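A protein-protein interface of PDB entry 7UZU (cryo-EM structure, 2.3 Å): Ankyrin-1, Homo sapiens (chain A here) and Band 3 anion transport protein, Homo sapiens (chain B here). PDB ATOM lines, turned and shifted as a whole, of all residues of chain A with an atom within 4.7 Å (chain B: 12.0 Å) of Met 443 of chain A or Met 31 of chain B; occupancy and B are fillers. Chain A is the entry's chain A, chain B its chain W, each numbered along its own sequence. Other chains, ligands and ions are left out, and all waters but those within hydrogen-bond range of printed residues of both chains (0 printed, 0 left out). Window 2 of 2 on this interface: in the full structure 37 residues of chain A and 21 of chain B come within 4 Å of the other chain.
NZ of Lys 380 of chain A sits close to O of Ser 29 of chain B (2.2 Å).
NZ of Lys 380 of chain A sits at hydrogen-bond distance from O of Glu 28 of chain B (3.3 Å).
NH1 of Arg 446 of chain A is in hydrogen-bond range of SD of Met 443 of chain A.
Among the printed residues, merely in contact across the chains: Met 443 of chain A with Met 31 of chain B (3.3 Å), Phe 413 of chain A with Met 31 of chain B (3.4 Å), Leu 405 of chain A with Met 31 of chain B (3.7 Å) and Val 410 of chain A with Met 31 of chain B (3.7 Å).
Leu 405 of chain A touches just one residue of chain B: Met 31 (3.7 Å).
No residue of chain B comes within 4 Å of Ser 412 of chain A.
Printed residues of chain B within 4 Å of Phe 413 of chain A: Met 31.
Thr 439 of chain A touches none of the printed residues of chain B.
Pro 440 of chain A touches none of the printed residues of chain B.
No residue of chain B comes within 4 Å of Leu 441 of chain A.
No residue of chain B comes within 4 Å of His 442 of chain A.
Met 443 of chain A touches just one residue of chain B: Met 31.
Ala 444 of chain A touches none of the printed residues of chain B.
No residue of chain B comes within 4 Å of Ala 447 of chain A.
Of the printed residues of chain A, Glu 28 of chain B touches Lys 380.
Of the printed residues of chain A, Ser 29 of chain B touches Lys 380 (2.2 Å).
Gln 30 of chain B touches none of the printed residues of chain A.
Of chain A, only Leu 405 (3.7 Å), Val 410 (3.7 Å), Phe 413 (3.4 Å) and Met 443 (3.3 Å) come within 4 Å of Met 31 of chain B.
The nearest residue of chain B that does not touch Met 443 of chain A is Glu 32 of chain B (7.5 Å).
The nearest printed residue of chain A that does not touch Glu 28 of chain B is Val 410 of chain A (9.5 Å).
Among the printed residues, 6 pairs touch across the chains.
Among the printed residues, no Asp or Glu carboxylate lies within 4 Å of a Lys or Arg side-chain nitrogen of the other chain.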
ATOM      1  N   LYS A 380      15.482   4.076   9.462  1.00  0.00           N
ATOM      2  CA  LYS A 380      16.741   4.731   9.126  1.00  0.00           C
ATOM      3  C   LYS A 380      17.896   3.737   9.103  1.00  0.00           C
ATOM      4  O   LYS A 380      18.751   3.788   8.212  1.00  0.00           O
ATOM      5  CB  LYS A 380      17.034   5.851  10.124  1.00  0.00           C
ATOM      6  CG  LYS A 380      18.321   6.596   9.835  1.00  0.00           C
ATOM      7  CD  LYS A 380      18.344   7.951  10.506  1.00  0.00           C
ATOM      8  CE  LYS A 380      19.564   8.746  10.085  1.00  0.00           C
ATOM      9  NZ  LYS A 380      20.388   9.150  11.256  1.00  0.00           N
ATOM     10  N   LEU A 405       8.764  14.130   8.068  1.00  0.00           N
ATOM     11  CA  LEU A 405       9.277  12.898   7.484  1.00  0.00           C
ATOM     12  C   LEU A 405       8.503  11.700   8.012  1.00  0.00           C
ATOM     13  O   LEU A 405       8.350  11.537   9.224  1.00  0.00           O
ATOM     14  CB  LEU A 405      10.760  12.730   7.812  1.00  0.00           C
ATOM     15  CG  LEU A 405      11.742  13.742   7.227  1.00  0.00           C
ATOM     16  CD1 LEU A 405      13.076  13.642   7.942  1.00  0.00           C
ATOM     17  CD2 LEU A 405      11.920  13.508   5.746  1.00  0.00           C
ATOM     18  N   HIS A 409       9.732   8.139   4.001  1.00  0.00           N
ATOM     19  CA  HIS A 409      10.708   9.169   3.660  1.00  0.00           C
ATOM     20  C   HIS A 409      12.106   8.754   4.094  1.00  0.00           C
ATOM     21  O   HIS A 409      13.061   8.806   3.311  1.00  0.00           O
ATOM     22  CB  HIS A 409      10.342  10.493   4.334  1.00  0.00           C
ATOM     23  CG  HIS A 409       9.396  11.343   3.550  1.00  0.00           C
ATOM     24  ND1 HIS A 409       8.043  11.378   3.805  1.00  0.00           N
ATOM     25  CD2 HIS A 409       9.611  12.210   2.532  1.00  0.00           C
ATOM     26  CE1 HIS A 409       7.462  12.223   2.972  1.00  0.00           C
ATOM     27  NE2 HIS A 409       8.391  12.740   2.188  1.00  0.00           N
ATOM     28  N   VAL A 410      12.236   8.350   5.357  1.00  0.00           N
ATOM     29  CA  VAL A 410      13.537   7.998   5.914  1.00  0.00           C
ATOM     30  C   VAL A 410      14.141   6.829   5.147  1.00  0.00           C
ATOM     31  O   VAL A 410      15.310   6.862   4.746  1.00  0.00           O
ATOM     32  CB  VAL A 410      13.390   7.677   7.413  1.00  0.00           C
ATOM     33  CG1 VAL A 410      14.632   7.021   7.953  1.00  0.00           C
ATOM     34  CG2 VAL A 410      13.065   8.938   8.194  1.00  0.00           C
ATOM     35  N   SER A 412      13.457   5.722   2.101  1.00  0.00           N
ATOM     36  CA  SER A 412      13.797   6.085   0.732  1.00  0.00           C
ATOM     37  C   SER A 412      15.076   6.906   0.685  1.00  0.00           C
ATOM     38  O   SER A 412      15.905   6.725  -0.213  1.00  0.00           O
ATOM     39  CB  SER A 412      12.643   6.852   0.090  1.00  0.00           C
ATOM     40  OG  SER A 412      11.543   5.996  -0.164  1.00  0.00           O
ATOM     41  N   PHE A 413      15.252   7.822   1.636  1.00  0.00           N
ATOM     42  CA  PHE A 413      16.478   8.606   1.662  1.00  0.00           C
ATOM     43  C   PHE A 413      17.691   7.724   1.928  1.00  0.00           C
ATOM     44  O   PHE A 413      18.734   7.882   1.282  1.00  0.00           O
ATOM     45  CB  PHE A 413      16.380   9.706   2.713  1.00  0.00           C
ATOM     46  CG  PHE A 413      17.586  10.584   2.770  1.00  0.00           C
ATOM     47  CD1 PHE A 413      17.868  11.458   1.737  1.00  0.00           C
ATOM     48  CD2 PHE A 413      18.446  10.531   3.852  1.00  0.00           C
ATOM     49  CE1 PHE A 413      18.980  12.268   1.787  1.00  0.00           C
ATOM     50  CE2 PHE A 413      19.559  11.337   3.905  1.00  0.00           C
ATOM     51  CZ  PHE A 413      19.827  12.207   2.870  1.00  0.00           C
ATOM     52  N   THR A 439       8.468  14.387  -1.576  1.00  0.00           N
ATOM     53  CA  THR A 439       7.934  13.054  -1.393  1.00  0.00           C
ATOM     54  C   THR A 439       9.065  12.055  -1.232  1.00  0.00           C
ATOM     55  O   THR A 439      10.242  12.395  -1.376  1.00  0.00           O
ATOM     56  CB  THR A 439       7.047  12.685  -2.583  1.00  0.00           C
ATOM     57  OG1 THR A 439       7.863  12.383  -3.722  1.00  0.00           O
ATOM     58  CG2 THR A 439       6.108  13.836  -2.919  1.00  0.00           C
ATOM     59  N   PRO A 440       8.749  10.803  -0.893  1.00  0.00           N
ATOM     60  CA  PRO A 440       9.799   9.773  -0.877  1.00  0.00           C
ATOM     61  C   PRO A 440      10.542   9.666  -2.194  1.00  0.00           C
ATOM     62  O   PRO A 440      11.747   9.391  -2.198  1.00  0.00           O
ATOM     63  CB  PRO A 440       9.020   8.492  -0.555  1.00  0.00           C
ATOM     64  CG  PRO A 440       7.848   8.948   0.216  1.00  0.00           C
ATOM     65  CD  PRO A 440       7.506  10.333  -0.259  1.00  0.00           C
ATOM     66  N   LEU A 441       9.851   9.867  -3.318  1.00  0.00           N
ATOM     67  CA  LEU A 441      10.520   9.827  -4.611  1.00  0.00           C
ATOM     68  C   LEU A 441      11.562  10.930  -4.732  1.00  0.00           C
ATOM     69  O   LEU A 441      12.639  10.699  -5.292  1.00  0.00           O
ATOM     70  CB  LEU A 441       9.492   9.934  -5.736  1.00  0.00           C
ATOM     71  CG  LEU A 441      10.032   9.855  -7.165  1.00  0.00           C
ATOM     72  CD1 LEU A 441      10.777   8.552  -7.402  1.00  0.00           C
ATOM     73  CD2 LEU A 441       8.895  10.014  -8.158  1.00  0.00           C
ATOM     74  N   HIS A 442      11.269  12.124  -4.213  1.00  0.00           N
ATOM     75  CA  HIS A 442      12.278  13.178  -4.180  1.00  0.00           C
ATOM     76  C   HIS A 442      13.499  12.735  -3.389  1.00  0.00           C
ATOM     77  O   HIS A 442      14.636  12.968  -3.811  1.00  0.00           O
ATOM     78  CB  HIS A 442      11.702  14.454  -3.565  1.00  0.00           C
ATOM     79  CG  HIS A 442      10.904  15.285  -4.517  1.00  0.00           C
ATOM     80  ND1 HIS A 442       9.525  15.290  -4.523  1.00  0.00           N
ATOM     81  CD2 HIS A 442      11.288  16.146  -5.489  1.00  0.00           C
ATOM     82  CE1 HIS A 442       9.095  16.114  -5.461  1.00  0.00           C
ATOM     83  NE2 HIS A 442      10.144  16.645  -6.062  1.00  0.00           N
ATOM     84  N   MET A 443      13.280  12.110  -2.234  1.00  0.00           N
ATOM     85  CA  MET A 443      14.394  11.684  -1.397  1.00  0.00           C
ATOM     86  C   MET A 443      15.222  10.610  -2.089  1.00  0.00           C
ATOM     87  O   MET A 443      16.454  10.622  -2.011  1.00  0.00           O
ATOM     88  CB  MET A 443      13.876  11.175  -0.050  1.00  0.00           C
ATOM     89  CG  MET A 443      12.938  12.137   0.668  1.00  0.00           C
ATOM     90  SD  MET A 443      13.810  13.463   1.512  1.00  0.00           S
ATOM     91  CE  MET A 443      13.796  12.839   3.182  1.00  0.00           C
ATOM     92  N   ALA A 444      14.561   9.666  -2.760  1.00  0.00           N
ATOM     93  CA  ALA A 444      15.287   8.643  -3.502  1.00  0.00           C
ATOM     94  C   ALA A 444      16.093   9.260  -4.635  1.00  0.00           C
ATOM     95  O   ALA A 444      17.250   8.887  -4.858  1.00  0.00           O
ATOM     96  CB  ALA A 444      14.314   7.596  -4.043  1.00  0.00           C
ATOM     97  N   ALA A 445      15.503  10.216  -5.357  1.00  0.00           N
ATOM     98  CA  ALA A 445      16.220  10.879  -6.442  1.00  0.00           C
ATOM     99  C   ALA A 445      17.433  11.632  -5.918  1.00  0.00           C
ATOM    100  O   ALA A 445      18.512  11.590  -6.518  1.00  0.00           O
ATOM    101  CB  ALA A 445      15.282  11.830  -7.184  1.00  0.00           C
ATOM    102  N   ARG A 446      17.273  12.331  -4.793  1.00  0.00           N
ATOM    103  CA  ARG A 446      18.355  13.154  -4.266  1.00  0.00           C
ATOM    104  C   ARG A 446      19.565  12.305  -3.900  1.00  0.00           C
ATOM    105  O   ARG A 446      20.708  12.698  -4.151  1.00  0.00           O
ATOM    106  CB  ARG A 446      17.861  13.939  -3.052  1.00  0.00           C
ATOM    107  CG  ARG A 446      18.781  15.066  -2.622  1.00  0.00           C
ATOM    108  CD  ARG A 446      18.062  16.088  -1.745  1.00  0.00           C
ATOM    109  NE  ARG A 446      18.533  16.040  -0.362  1.00  0.00           N
ATOM    110  CZ  ARG A 446      17.781  15.797   0.706  1.00  0.00           C
ATOM    111  NH1 ARG A 446      16.477  15.578   0.612  1.00  0.00           N
ATOM    112  NH2 ARG A 446      18.352  15.779   1.907  1.00  0.00           N
ATOM    113  N   ALA A 447      19.331  11.139  -3.303  1.00  0.00           N
ATOM    114  CA  ALA A 447      20.397  10.224  -2.926  1.00  0.00           C
ATOM    115  C   ALA A 447      20.761   9.248  -4.037  1.00  0.00           C
ATOM    116  O   ALA A 447      21.666   8.429  -3.850  1.00  0.00           O
ATOM    117  CB  ALA A 447      19.995   9.446  -1.671  1.00  0.00           C
ATOM    118  N   ILE B  26      25.394   9.824  22.837  1.00  0.00           N
ATOM    119  CA  ILE B  26      24.065   9.437  22.372  1.00  0.00           C
ATOM    120  C   ILE B  26      23.952   9.851  20.911  1.00  0.00           C
ATOM    121  O   ILE B  26      23.397  10.920  20.616  1.00  0.00           O
ATOM    122  CB  ILE B  26      22.962  10.084  23.224  1.00  0.00           C
ATOM    123  N   PRO B  27      24.458   9.058  19.967  1.00  0.00           N
ATOM    124  CA  PRO B  27      24.485   9.506  18.572  1.00  0.00           C
ATOM    125  C   PRO B  27      23.088   9.707  18.010  1.00  0.00           C
ATOM    126  O   PRO B  27      22.142   8.993  18.350  1.00  0.00           O
ATOM    127  CB  PRO B  27      25.219   8.373  17.846  1.00  0.00           C
ATOM    128  CG  PRO B  27      24.996   7.175  18.690  1.00  0.00           C
ATOM    129  CD  PRO B  27      24.916   7.664  20.108  1.00  0.00           C
ATOM    130  N   GLU B  28      22.973  10.700  17.134  1.00  0.00           N
ATOM    131  CA  GLU B  28      21.724  11.024  16.455  1.00  0.00           C
ATOM    132  C   GLU B  28      21.817  10.874  14.947  1.00  0.00           C
ATOM    133  O   GLU B  28      20.870  10.390  14.322  1.00  0.00           O
ATOM    134  CB  GLU B  28      21.294  12.458  16.796  1.00  0.00           C
ATOM    135  N   SER B  29      22.938  11.271  14.345  1.00  0.00           N
ATOM    136  CA  SER B  29      23.147  11.148  12.906  1.00  0.00           C
ATOM    137  C   SER B  29      22.025  11.846  12.138  1.00  0.00           C
ATOM    138  O   SER B  29      21.226  11.221  11.438  1.00  0.00           O
ATOM    139  CB  SER B  29      23.261   9.677  12.498  1.00  0.00           C
ATOM    140  N   GLN B  30      21.970  13.168  12.301  1.00  0.00           N
ATOM    141  CA  GLN B  30      20.941  13.982  11.664  1.00  0.00           C
ATOM    142  C   GLN B  30      20.828  13.650  10.183  1.00  0.00           C
ATOM    143  O   GLN B  30      21.810  13.714   9.440  1.00  0.00           O
ATOM    144  CB  GLN B  30      21.266  15.467  11.847  1.00  0.00           C
ATOM    145  N   MET B  31      19.614  13.287   9.762  1.00  0.00           N
ATOM    146  CA  MET B  31      19.412  12.846   8.385  1.00  0.00           C
ATOM    147  C   MET B  31      19.726  13.962   7.397  1.00  0.00           C
ATOM    148  O   MET B  31      20.341  13.721   6.352  1.00  0.00           O
ATOM    149  CB  MET B  31      17.979  12.351   8.203  1.00  0.00           C
ATOM    150  CG  MET B  31      17.805  11.404   7.031  1.00  0.00           C
ATOM    151  SD  MET B  31      16.187  10.613   7.002  1.00  0.00           S
ATOM    152  CE  MET B  31      15.329  11.643   5.819  1.00  0.00           C
ATOM    153  N   GLU B  32      19.312  15.187   7.707  1.00  0.00           N
ATOM    154  CA  GLU B  32      19.603  16.322   6.849  1.00  0.00           C
ATOM    155  C   GLU B  32      21.069  16.723   6.993  1.00  0.00           C
ATOM    156  O   GLU B  32      21.847  16.096   7.719  1.00  0.00           O
ATOM    157  CB  GLU B  32      18.677  17.491   7.185  1.00  0.00           C
ATOM    158  N   GLU B  33      21.455  17.782   6.290  1.00  0.00           N
ATOM    159  CA  GLU B  33      22.829  18.267   6.332  1.00  0.00           C
ATOM    160  C   GLU B  33      22.897  19.738   5.939  1.00  0.00           C
ATOM    161  O   GLU B  33      23.862  20.433   6.260  1.00  0.00           O
ATOM    162  CB  GLU B  33      23.719  17.435   5.408  1.00  0.00           C
